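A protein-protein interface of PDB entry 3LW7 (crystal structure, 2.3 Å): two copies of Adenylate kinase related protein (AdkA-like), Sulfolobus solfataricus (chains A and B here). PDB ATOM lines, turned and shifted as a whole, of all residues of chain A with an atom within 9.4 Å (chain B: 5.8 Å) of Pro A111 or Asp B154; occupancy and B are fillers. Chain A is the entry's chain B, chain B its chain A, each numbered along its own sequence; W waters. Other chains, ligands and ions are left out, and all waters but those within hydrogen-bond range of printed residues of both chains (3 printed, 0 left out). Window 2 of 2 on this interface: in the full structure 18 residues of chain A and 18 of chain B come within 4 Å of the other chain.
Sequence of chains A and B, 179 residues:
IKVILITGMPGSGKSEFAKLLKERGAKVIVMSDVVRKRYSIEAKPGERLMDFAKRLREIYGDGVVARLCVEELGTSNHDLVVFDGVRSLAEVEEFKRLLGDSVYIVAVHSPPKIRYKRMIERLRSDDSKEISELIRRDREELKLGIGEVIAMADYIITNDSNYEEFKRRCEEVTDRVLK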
ATOM      1  N   MET A   9       9.479 -21.406  15.506  1.00  0.00           N
ATOM      2  CA  MET A   9       8.472 -21.910  14.547  1.00  0.00           C
ATOM      3  C   MET A   9       7.660 -23.075  15.134  1.00  0.00           C
ATOM      4  O   MET A   9       8.066 -23.655  16.141  1.00  0.00           O
ATOM      5  CB  MET A   9       9.142 -22.276  13.197  1.00  0.00           C
ATOM      6  CG  MET A   9       9.857 -21.047  12.513  1.00  0.00           C
ATOM      7  SD  MET A   9       8.704 -19.806  11.849  1.00  0.00           S
ATOM      8  CE  MET A   9       8.007 -20.673  10.453  1.00  0.00           C
ATOM      9  N   PRO A  10       6.489 -23.393  14.536  1.00  0.00           N
ATOM     10  CA  PRO A  10       5.682 -24.541  14.991  1.00  0.00           C
ATOM     11  C   PRO A  10       6.465 -25.853  14.947  1.00  0.00           C
ATOM     12  O   PRO A  10       7.135 -26.155  13.952  1.00  0.00           O
ATOM     13  CB  PRO A  10       4.530 -24.593  13.974  1.00  0.00           C
ATOM     14  CG  PRO A  10       4.452 -23.226  13.400  1.00  0.00           C
ATOM     15  CD  PRO A  10       5.834 -22.655  13.427  1.00  0.00           C
ATOM     16  N   GLY A  11       6.388 -26.612  16.031  1.00  0.00           N
ATOM     17  CA  GLY A  11       7.136 -27.863  16.173  1.00  0.00           C
ATOM     18  C   GLY A  11       8.619 -27.721  16.478  1.00  0.00           C
ATOM     19  O   GLY A  11       9.357 -28.687  16.361  1.00  0.00           O
ATOM     20  N   SER A  12       9.054 -26.525  16.868  1.00  0.00           N
ATOM     21  CA  SER A  12      10.465 -26.231  17.119  1.00  0.00           C
ATOM     22  C   SER A  12      10.941 -26.723  18.480  1.00  0.00           C
ATOM     23  O   SER A  12      12.133 -26.919  18.685  1.00  0.00           O
ATOM     24  CB  SER A  12      10.696 -24.714  17.058  1.00  0.00           C
ATOM     25  OG  SER A  12       9.882 -24.049  18.037  1.00  0.00           O
ATOM     26  N   GLY A  13      10.011 -26.899  19.411  1.00  0.00           N
ATOM     27  CA  GLY A  13      10.355 -27.244  20.800  1.00  0.00           C
ATOM     28  C   GLY A  13      10.558 -26.014  21.683  1.00  0.00           C
ATOM     29  O   GLY A  13      11.152 -26.112  22.771  1.00  0.00           O
ATOM     30  N   VAL A 108      14.167 -20.594  19.675  1.00  0.00           N
ATOM     31  CA  VAL A 108      14.443 -22.022  19.546  1.00  0.00           C
ATOM     32  C   VAL A 108      14.349 -22.342  18.051  1.00  0.00           C
ATOM     33  O   VAL A 108      13.299 -22.123  17.420  1.00  0.00           O
ATOM     34  CB  VAL A 108      13.495 -22.883  20.397  1.00  0.00           C
ATOM     35  CG1 VAL A 108      13.745 -24.362  20.136  1.00  0.00           C
ATOM     36  CG2 VAL A 108      13.729 -22.589  21.908  1.00  0.00           C
ATOM     37  N   HIS A 109      15.459 -22.804  17.482  1.00  0.00           N
ATOM     38  CA  HIS A 109      15.492 -23.210  16.077  1.00  0.00           C
ATOM     39  C   HIS A 109      15.469 -24.725  15.849  1.00  0.00           C
ATOM     40  O   HIS A 109      16.191 -25.480  16.528  1.00  0.00           O
ATOM     41  CB  HIS A 109      16.716 -22.611  15.365  1.00  0.00           C
ATOM     42  CG  HIS A 109      16.784 -22.980  13.921  1.00  0.00           C
ATOM     43  ND1 HIS A 109      15.909 -22.465  12.987  1.00  0.00           N
ATOM     44  CD2 HIS A 109      17.578 -23.856  13.256  1.00  0.00           C
ATOM     45  CE1 HIS A 109      16.169 -22.994  11.806  1.00  0.00           C
ATOM     46  NE2 HIS A 109      17.176 -23.841  11.941  1.00  0.00           N
ATOM     47  N   SER A 110      14.631 -25.156  14.911  1.00  0.00           N
ATOM     48  CA  SER A 110      14.703 -26.485  14.286  1.00  0.00           C
ATOM     49  C   SER A 110      14.474 -26.306  12.786  1.00  0.00           C
ATOM     50  O   SER A 110      13.618 -25.525  12.398  1.00  0.00           O
ATOM     51  CB  SER A 110      13.592 -27.400  14.795  1.00  0.00           C
ATOM     52  OG  SER A 110      13.927 -27.996  16.015  1.00  0.00           O
ATOM     53  N   PRO A 111      15.206 -27.062  11.937  1.00  0.00           N
ATOM     54  CA  PRO A 111      15.031 -26.904  10.487  1.00  0.00           C
ATOM     55  C   PRO A 111      13.669 -27.422  10.047  1.00  0.00           C
ATOM     56  O   PRO A 111      13.131 -28.307  10.702  1.00  0.00           O
ATOM     57  CB  PRO A 111      16.150 -27.775   9.877  1.00  0.00           C
ATOM     58  CG  PRO A 111      16.587 -28.684  10.924  1.00  0.00           C
ATOM     59  CD  PRO A 111      16.203 -28.094  12.277  1.00  0.00           C
ATOM     60  N   PRO A 112      13.117 -26.882   8.946  1.00  0.00           N
ATOM     61  CA  PRO A 112      11.752 -27.217   8.469  1.00  0.00           C
ATOM     62  C   PRO A 112      11.439 -28.722   8.398  1.00  0.00           C
ATOM     63  O   PRO A 112      10.425 -29.171   8.960  1.00  0.00           O
ATOM     64  CB  PRO A 112      11.706 -26.623   7.062  1.00  0.00           C
ATOM     65  CG  PRO A 112      12.715 -25.490   7.085  1.00  0.00           C
ATOM     66  CD  PRO A 112      13.766 -25.845   8.119  1.00  0.00           C
ATOM     67  N   LYS A 113      12.291 -29.497   7.724  1.00  0.00           N
ATOM     68  CA  LYS A 113      12.031 -30.929   7.565  1.00  0.00           C
ATOM     69  C   LYS A 113      11.995 -31.655   8.911  1.00  0.00           C
ATOM     70  O   LYS A 113      11.230 -32.600   9.085  1.00  0.00           O
ATOM     71  CB  LYS A 113      13.033 -31.589   6.609  1.00  0.00           C
ATOM     72  CG  LYS A 113      12.855 -31.168   5.152  1.00  0.00           C
ATOM     73  CD  LYS A 113      13.926 -31.779   4.256  1.00  0.00           C
ATOM     74  CE  LYS A 113      13.629 -31.503   2.788  1.00  0.00           C
ATOM     75  NZ  LYS A 113      14.555 -32.242   1.873  1.00  0.00           N
ATOM     76  N   ILE A 114      12.809 -31.215   9.866  1.00  0.00           N
ATOM     77  CA  ILE A 114      12.766 -31.825  11.200  1.00  0.00           C
ATOM     78  C   ILE A 114      11.476 -31.502  11.939  1.00  0.00           C
ATOM     79  O   ILE A 114      10.830 -32.409  12.469  1.00  0.00           O
ATOM     80  CB  ILE A 114      14.032 -31.563  12.036  1.00  0.00           C
ATOM     81  CG1 ILE A 114      15.139 -32.515  11.572  1.00  0.00           C
ATOM     82  CG2 ILE A 114      13.748 -31.801  13.499  1.00  0.00           C
ATOM     83  CD1 ILE A 114      16.482 -32.287  12.231  1.00  0.00           C
ATOM     84  N   ARG A 115      11.046 -30.267  11.892  1.00  0.00           N
ATOM     85  CA  ARG A 115       9.846 -29.851  12.550  1.00  0.00           C
ATOM     86  C   ARG A 115       8.634 -30.482  11.941  1.00  0.00           C
ATOM     87  O   ARG A 115       7.714 -30.782  12.622  1.00  0.00           O
ATOM     88  CB  ARG A 115       9.668 -28.348  12.489  1.00  0.00           C
ATOM     89  CG  ARG A 115      10.645 -27.542  13.272  1.00  0.00           C
ATOM     90  CD  ARG A 115      10.227 -26.115  13.287  1.00  0.00           C
ATOM     91  NE  ARG A 115      10.411 -25.515  12.001  1.00  0.00           N
ATOM     92  CZ  ARG A 115       9.461 -25.089  11.205  1.00  0.00           C
ATOM     93  NH1 ARG A 115       9.776 -24.573  10.063  1.00  0.00           N
ATOM     94  NH2 ARG A 115       8.222 -25.182  11.533  1.00  0.00           N
ATOM     95  N   TYR A 116       8.615 -30.618  10.633  1.00  0.00           N
ATOM     96  CA  TYR A 116       7.510 -31.317   9.969  1.00  0.00           C
ATOM     97  C   TYR A 116       7.484 -32.796  10.332  1.00  0.00           C
ATOM     98  O   TYR A 116       6.407 -33.379  10.563  1.00  0.00           O
ATOM     99  CB  TYR A 116       7.525 -31.161   8.437  1.00  0.00           C
ATOM    100  CG  TYR A 116       7.508 -29.741   7.912  1.00  0.00           C
ATOM    101  CD1 TYR A 116       6.960 -28.695   8.649  1.00  0.00           C
ATOM    102  CD2 TYR A 116       8.056 -29.449   6.650  1.00  0.00           C
ATOM    103  CE1 TYR A 116       6.967 -27.382   8.147  1.00  0.00           C
ATOM    104  CE2 TYR A 116       8.065 -28.155   6.143  1.00  0.00           C
ATOM    105  CZ  TYR A 116       7.519 -27.129   6.887  1.00  0.00           C
ATOM    106  OH  TYR A 116       7.544 -25.858   6.361  1.00  0.00           O
ATOM    107  N   LYS A 117       8.665 -33.404  10.387  1.00  0.00           N
ATOM    108  CA  LYS A 117       8.775 -34.802  10.786  1.00  0.00           C
ATOM    109  C   LYS A 117       8.202 -35.040  12.185  1.00  0.00           C
ATOM    110  O   LYS A 117       7.560 -36.053  12.411  1.00  0.00           O
ATOM    111  CB  LYS A 117      10.230 -35.294  10.707  1.00  0.00           C
ATOM    112  CG  LYS A 117      10.377 -36.804  10.751  1.00  0.00           C
ATOM    113  CD  LYS A 117      11.833 -37.244  10.697  1.00  0.00           C
ATOM    114  CE  LYS A 117      11.955 -38.744  10.958  1.00  0.00           C
ATOM    115  NZ  LYS A 117      13.319 -39.256  10.652  1.00  0.00           N
ATOM    116  N   ARG A 118       8.438 -34.112  13.115  1.00  0.00           N
ATOM    117  CA  ARG A 118       7.912 -34.243  14.486  1.00  0.00           C
ATOM    118  C   ARG A 118       6.393 -34.132  14.521  1.00  0.00           C
ATOM    119  O   ARG A 118       5.724 -34.947  15.167  1.00  0.00           O
ATOM    120  CB  ARG A 118       8.513 -33.208  15.448  1.00  0.00           C
ATOM    121  CG  ARG A 118       9.939 -33.471  15.909  1.00  0.00           C
ATOM    122  CD  ARG A 118      10.462 -32.238  16.642  1.00  0.00           C
ATOM    123  NE  ARG A 118      11.906 -32.273  16.876  1.00  0.00           N
ATOM    124  CZ  ARG A 118      12.675 -31.192  16.930  1.00  0.00           C
ATOM    125  NH1 ARG A 118      12.148 -29.980  16.746  1.00  0.00           N
ATOM    126  NH2 ARG A 118      13.979 -31.316  17.153  1.00  0.00           N
ATOM    127  N   MET A 119       5.854 -33.130  13.825  1.00  0.00           N
ATOM    128  CA  MET A 119       4.407 -32.870  13.847  1.00  0.00           C
ATOM    129  C   MET A 119       3.566 -33.987  13.206  1.00  0.00           C
ATOM    130  O   MET A 119       2.448 -34.236  13.645  1.00  0.00           O
ATOM    131  CB  MET A 119       4.081 -31.497  13.241  1.00  0.00           C
ATOM    132  CG  MET A 119       4.596 -30.314  14.090  1.00  0.00           C
ATOM    133  SD  MET A 119       4.179 -28.650  13.505  1.00  0.00           S
ATOM    134  CE  MET A 119       5.270 -28.497  12.087  1.00  0.00           C
ATOM    135  N   ASP A 138       3.343 -22.413   8.487  1.00  0.00           N
ATOM    136  CA  ASP A 138       4.633 -21.752   8.513  1.00  0.00           C
ATOM    137  C   ASP A 138       4.574 -20.394   7.778  1.00  0.00           C
ATOM    138  O   ASP A 138       4.974 -19.364   8.329  1.00  0.00           O
ATOM    139  CB  ASP A 138       5.703 -22.645   7.866  1.00  0.00           C
ATOM    140  CG  ASP A 138       6.354 -23.595   8.846  1.00  0.00           C
ATOM    141  OD1 ASP A 138       5.891 -23.714   9.999  1.00  0.00           O
ATOM    142  OD2 ASP A 138       7.359 -24.236   8.460  1.00  0.00           O
ATOM    143  N   ILE A 157      18.908 -21.083  20.228  1.00  0.00           N
ATOM    144  CA  ILE A 157      19.161 -22.443  20.668  1.00  0.00           C
ATOM    145  C   ILE A 157      18.684 -23.382  19.569  1.00  0.00           C
ATOM    146  O   ILE A 157      17.509 -23.347  19.194  1.00  0.00           O
ATOM    147  CB  ILE A 157      18.357 -22.730  21.957  1.00  0.00           C
ATOM    148  CG1 ILE A 157      18.800 -21.789  23.087  1.00  0.00           C
ATOM    149  CG2 ILE A 157      18.497 -24.197  22.391  1.00  0.00           C
ATOM    150  CD1 ILE A 157      17.899 -21.873  24.332  1.00  0.00           C
ATOM    151  N   THR A 158      19.574 -24.229  19.050  1.00  0.00           N
ATOM    152  CA  THR A 158      19.120 -25.246  18.106  1.00  0.00           C
ATOM    153  C   THR A 158      18.747 -26.598  18.732  1.00  0.00           C
ATOM    154  O   THR A 158      19.491 -27.184  19.524  1.00  0.00           O
ATOM    155  CB  THR A 158      19.931 -25.351  16.760  1.00  0.00           C
ATOM    156  OG1 THR A 158      20.381 -26.699  16.549  1.00  0.00           O
ATOM    157  CG2 THR A 158      21.080 -24.373  16.674  1.00  0.00           C
ATOM    158  N   ASN A 159      17.547 -27.038  18.378  1.00  0.00           N
ATOM    159  CA  ASN A 159      16.976 -28.299  18.813  1.00  0.00           C
ATOM    160  C   ASN A 159      16.925 -29.224  17.601  1.00  0.00           C
ATOM    161  O   ASN A 159      15.941 -29.227  16.869  1.00  0.00           O
ATOM    162  CB  ASN A 159      15.558 -28.049  19.362  1.00  0.00           C
ATOM    163  CG  ASN A 159      14.802 -29.339  19.671  1.00  0.00           C
ATOM    164  OD1 ASN A 159      15.394 -30.413  19.803  1.00  0.00           O
ATOM    165  ND2 ASN A 159      13.490 -29.236  19.775  1.00  0.00           N
ATOM    166  N   ASP A 160      17.995 -29.975  17.352  1.00  0.00           N
ATOM    167  CA  ASP A 160      18.028 -30.842  16.169  1.00  0.00           C
ATOM    168  C   ASP A 160      18.675 -32.211  16.394  1.00  0.00           C
ATOM    169  O   ASP A 160      18.837 -32.997  15.455  1.00  0.00           O
ATOM    170  CB  ASP A 160      18.609 -30.103  14.935  1.00  0.00           C
ATOM    171  CG  ASP A 160      20.156 -29.987  14.947  1.00  0.00           C
ATOM    172  OD1 ASP A 160      20.828 -30.379  15.954  1.00  0.00           O
ATOM    173  OD2 ASP A 160      20.692 -29.487  13.917  1.00  0.00           O
ATOM    174  N   SER A 161      19.050 -32.481  17.638  1.00  0.00           N
ATOM    175  CA  SER A 161      19.626 -33.762  18.032  1.00  0.00           C
ATOM    176  C   SER A 161      18.640 -34.467  18.969  1.00  0.00           C
ATOM    177  O   SER A 161      17.497 -34.714  18.593  1.00  0.00           O
ATOM    178  CB  SER A 161      20.975 -33.535  18.725  1.00  0.00           C
ATOM    179  OG  SER A 161      20.815 -32.717  19.878  1.00  0.00           O
ATOM    180  N   ARG A 169      21.893 -27.099  26.292  1.00  0.00           N
ATOM    181  CA  ARG A 169      21.924 -25.813  25.568  1.00  0.00           C
ATOM    182  C   ARG A 169      20.974 -24.766  26.161  1.00  0.00           C
ATOM    183  O   ARG A 169      21.352 -23.607  26.292  1.00  0.00           O
ATOM    184  CB  ARG A 169      21.642 -26.018  24.082  1.00  0.00           C
ATOM    185  CG  ARG A 169      22.801 -26.677  23.338  1.00  0.00           C
ATOM    186  CD  ARG A 169      22.314 -27.348  22.065  1.00  0.00           C
ATOM    187  NE  ARG A 169      23.405 -27.890  21.266  1.00  0.00           N
ATOM    188  CZ  ARG A 169      23.251 -28.418  20.053  1.00  0.00           C
ATOM    189  NH1 ARG A 169      22.042 -28.474  19.494  1.00  0.00           N
ATOM    190  NH2 ARG A 169      24.304 -28.896  19.395  1.00  0.00           N
ATOM    191  N   LYS B  96      16.807 -23.685  -5.683  1.00  0.00           N
ATOM    192  CA  LYS B  96      16.261 -25.053  -5.693  1.00  0.00           C
ATOM    193  C   LYS B  96      15.726 -25.496  -7.058  1.00  0.00           C
ATOM    194  O   LYS B  96      15.959 -26.631  -7.463  1.00  0.00           O
ATOM    195  CB  LYS B  96      15.206 -25.249  -4.604  1.00  0.00           C
ATOM    196  CG  LYS B  96      15.772 -25.084  -3.197  1.00  0.00           C
ATOM    197  CD  LYS B  96      14.867 -25.622  -2.094  1.00  0.00           C
ATOM    198  CE  LYS B  96      15.521 -25.248  -0.774  1.00  0.00           C
ATOM    199  NZ  LYS B  96      15.191 -26.071   0.408  1.00  0.00           N
ATOM    200  N   VAL B 103      20.302 -28.511  -1.804  1.00  0.00           N
ATOM    201  CA  VAL B 103      20.525 -27.112  -1.439  1.00  0.00           C
ATOM    202  C   VAL B 103      20.225 -26.870   0.055  1.00  0.00           C
ATOM    203  O   VAL B 103      19.164 -27.241   0.559  1.00  0.00           O
ATOM    204  CB  VAL B 103      19.648 -26.181  -2.298  1.00  0.00           C
ATOM    205  CG1 VAL B 103      19.902 -24.719  -1.968  1.00  0.00           C
ATOM    206  CG2 VAL B 103      19.892 -26.440  -3.789  1.00  0.00           C
ATOM    207  N   TYR B 104      21.166 -26.245   0.753  1.00  0.00           N
ATOM    208  CA  TYR B 104      21.055 -26.037   2.184  1.00  0.00           C
ATOM    209  C   TYR B 104      21.244 -24.586   2.551  1.00  0.00           C
ATOM    210  O   TYR B 104      22.114 -23.906   2.009  1.00  0.00           O
ATOM    211  CB  TYR B 104      22.120 -26.849   2.911  1.00  0.00           C
ATOM    212  CG  TYR B 104      22.066 -28.305   2.585  1.00  0.00           C
ATOM    213  CD1 TYR B 104      22.831 -28.830   1.544  1.00  0.00           C
ATOM    214  CD2 TYR B 104      21.224 -29.160   3.295  1.00  0.00           C
ATOM    215  CE1 TYR B 104      22.773 -30.172   1.225  1.00  0.00           C
ATOM    216  CE2 TYR B 104      21.157 -30.516   2.985  1.00  0.00           C
ATOM    217  CZ  TYR B 104      21.942 -31.011   1.950  1.00  0.00           C
ATOM    218  OH  TYR B 104      21.899 -32.340   1.642  1.00  0.00           O
ATOM    219  N   ILE B 105      20.450 -24.126   3.502  1.00  0.00           N
ATOM    220  CA  ILE B 105      20.575 -22.783   4.003  1.00  0.00           C
ATOM    221  C   ILE B 105      21.390 -22.837   5.296  1.00  0.00           C
ATOM    222  O   ILE B 105      21.053 -23.591   6.218  1.00  0.00           O
ATOM    223  CB  ILE B 105      19.180 -22.152   4.281  1.00  0.00           C
ATOM    224  CG1 ILE B 105      18.337 -22.094   3.008  1.00  0.00           C
ATOM    225  CG2 ILE B 105      19.305 -20.761   4.923  1.00  0.00           C
ATOM    226  CD1 ILE B 105      16.819 -22.174   3.306  1.00  0.00           C
ATOM    227  N   VAL B 106      22.470 -22.054   5.361  1.00  0.00           N
ATOM    228  CA  VAL B 106      23.206 -21.921   6.625  1.00  0.00           C
ATOM    229  C   VAL B 106      23.160 -20.462   7.049  1.00  0.00           C
ATOM    230  O   VAL B 106      23.671 -19.592   6.335  1.00  0.00           O
ATOM    231  CB  VAL B 106      24.686 -22.362   6.504  1.00  0.00           C
ATOM    232  CG1 VAL B 106      25.449 -22.027   7.775  1.00  0.00           C
ATOM    233  CG2 VAL B 106      24.799 -23.850   6.174  1.00  0.00           C
ATOM    234  N   MET B 152      13.921 -20.427   8.404  1.00  0.00           N
ATOM    235  CA  MET B 152      13.756 -21.683   7.672  1.00  0.00           C
ATOM    236  C   MET B 152      15.089 -22.392   7.377  1.00  0.00           C
ATOM    237  O   MET B 152      15.158 -23.298   6.541  1.00  0.00           O
ATOM    238  CB  MET B 152      12.988 -21.400   6.369  1.00  0.00           C
ATOM    239  CG  MET B 152      11.575 -20.798   6.617  1.00  0.00           C
ATOM    240  SD  MET B 152      10.401 -21.912   7.459  1.00  0.00           S
ATOM    241  CE  MET B 152      10.092 -23.025   6.101  1.00  0.00           C
ATOM    242  N   ALA B 153      16.148 -21.977   8.066  1.00  0.00           N
ATOM    243  CA  ALA B 153      17.488 -22.485   7.817  1.00  0.00           C
ATOM    244  C   ALA B 153      17.657 -23.938   8.203  1.00  0.00           C
ATOM    245  O   ALA B 153      17.053 -24.407   9.167  1.00  0.00           O
ATOM    246  CB  ALA B 153      18.515 -21.634   8.571  1.00  0.00           C
ATOM    247  N   ASP B 154      18.510 -24.634   7.462  1.00  0.00           N
ATOM    248  CA  ASP B 154      18.938 -25.975   7.841  1.00  0.00           C
ATOM    249  C   ASP B 154      19.879 -25.960   9.051  1.00  0.00           C
ATOM    250  O   ASP B 154      19.872 -26.890   9.847  1.00  0.00           O
ATOM    251  CB  ASP B 154      19.591 -26.674   6.648  1.00  0.00           C
ATOM    252  CG  ASP B 154      18.622 -26.852   5.513  1.00  0.00           C
ATOM    253  OD1 ASP B 154      18.590 -26.004   4.604  1.00  0.00           O
ATOM    254  OD2 ASP B 154      17.827 -27.808   5.566  1.00  0.00           O
ATOM    255  N   TYR B 155      20.691 -24.913   9.158  1.00  0.00           N
ATOM    256  CA  TYR B 155      21.679 -24.783  10.218  1.00  0.00           C
ATOM    257  C   TYR B 155      21.839 -23.315  10.563  1.00  0.00           C
ATOM    258  O   TYR B 155      21.885 -22.454   9.674  1.00  0.00           O
ATOM    259  CB  TYR B 155      23.039 -25.373   9.799  1.00  0.00           C
ATOM    260  CG  TYR B 155      22.993 -26.869   9.521  1.00  0.00           C
ATOM    261  CD1 TYR B 155      23.024 -27.802  10.572  1.00  0.00           C
ATOM    262  CD2 TYR B 155      22.875 -27.355   8.216  1.00  0.00           C
ATOM    263  CE1 TYR B 155      22.958 -29.189  10.316  1.00  0.00           C
ATOM    264  CE2 TYR B 155      22.799 -28.733   7.957  1.00  0.00           C
ATOM    265  CZ  TYR B 155      22.846 -29.638   9.009  1.00  0.00           C
ATOM    266  OH  TYR B 155      22.783 -30.995   8.754  1.00  0.00           O
ATOM    267  N   ILE B 156      21.903 -23.040  11.859  1.00  0.00           N
ATOM    268  CA  ILE B 156      22.207 -21.712  12.337  1.00  0.00           C
ATOM    269  C   ILE B 156      23.472 -21.781  13.176  1.00  0.00           C
ATOM    270  O   ILE B 156      23.549 -22.551  14.150  1.00  0.00           O
ATOM    271  CB  ILE B 156      21.023 -21.091  13.134  1.00  0.00           C
ATOM    272  CG1 ILE B 156      19.874 -20.785  12.163  1.00  0.00           C
ATOM    273  CG2 ILE B 156      21.491 -19.828  13.823  1.00  0.00           C
ATOM    274  CD1 ILE B 156      18.585 -20.209  12.770  1.00  0.00           C
HETATM  275  O   HOH W   1      21.380 -25.249  13.619  1.00  0.00           O
HETATM  276  O   HOH W   2      19.878 -27.045  12.683  1.00  0.00           O
HETATM  277  O   HOH W   3      14.812 -28.656   6.685  1.00  0.00           O
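The backbone carbonyl oxygen (O) of Ile A157 sits at hydrogen-bond distance from the backbone NH (N) of His A109 (2.7 Å).
O of Pro A10 lies within hydrogen-bond range of NH2 of Arg A115.
N of Ile B105 sits at hydrogen-bond distance from OD1 of Asp B154 (2.9 Å).
The backbone carbonyl oxygen (O) of Thr A158 lies within hydrogen-bond range of the guanidinium group (NH1) of Arg A169 (2.9 Å).
The backbone NH of Asn A159 lies within hydrogen-bond range of the backbone carbonyl oxygen of His A109, at 2.8 Å.
NH1 of Arg A115 is in salt-bridge range of OD2 of Asp A138, at 2.9 Å.
Water W2 bridges O of Asp B154 (2.8 Å) and OD2 of Asp A160 (2.9 Å).
Water W3 lies within hydrogen-bond range of the backbone NH of Lys A113 and the side-chain carboxylate of Asp B154.
Water W1 bridges N of Ile B156 and OG1 of Thr A158.
His A109 touches Ile B156 (CG to CD1, 3.5 Å).
O of Ala B153 touches CA of Pro A111, at 3.5 Å.
Pro A111 touches Asp B154.
Met B152 touches Pro A112.
Pro A112 touches Ala B153.
Tyr A116 touches Met B152.
Asp A138 touches Met B152.
Thr A158 touches Ile B156.
No position is printed for both chains.
Met A9 touches none of the printed residues of chain B.
Pro A111 touches just these residues of chain B: Ala B153 (3.5 Å) and Asp B154 (3.8 Å).
Of the printed residues of chain B, Arg A115 touches Met B152.
Met A119 touches none of the printed residues of chain B.
Of the printed residues of chain B, Thr A158 touches Ile B156 (3.97 Å).
Ile B105 touches none of the printed residues of chain A.
Of the printed residues of chain A, Met B152 touches Pro A112, Arg A115, Tyr A116 and Asp A138.
Of chain A, only His A109, Pro A111 and Pro A112 come within 4 Å of Ala B153.
Of chain A, only Pro A111 (3.8 Å) comes within 4 Å of Asp B154.
Of the printed residues of chain A, Ile B156 touches His A109 (3.5 Å) and Thr A158 (3.97 Å).
The nearest printed residue of chain B that does not touch Thr A158 is Tyr B155 (6.2 Å).
SD of Met B152 is in hydrogen-bond range of NH1 of Arg A115 (3.8 Å).
The backbone carbonyl oxygen (O) of Ala B153 lies within hydrogen-bond range of a ring nitrogen (NE2) of His A109, at 2.8 Å.
Printed residues of chain B that touch a printed residue of chain A: Met B152, Ala B153, Asp B154 and Ile B156.
Of the 24 printed residues of chain A, 7 touch a printed residue of chain B.
Along chain A the printed residues that touch a printed residue of chain B span positions 109 to 158.
Among the printed residues, 10 pairs touch across the chains.
Among the printed residues, no Asp or Glu carboxylate lies within 4 Å of a Lys or Arg side-chain nitrogen of the other chain.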
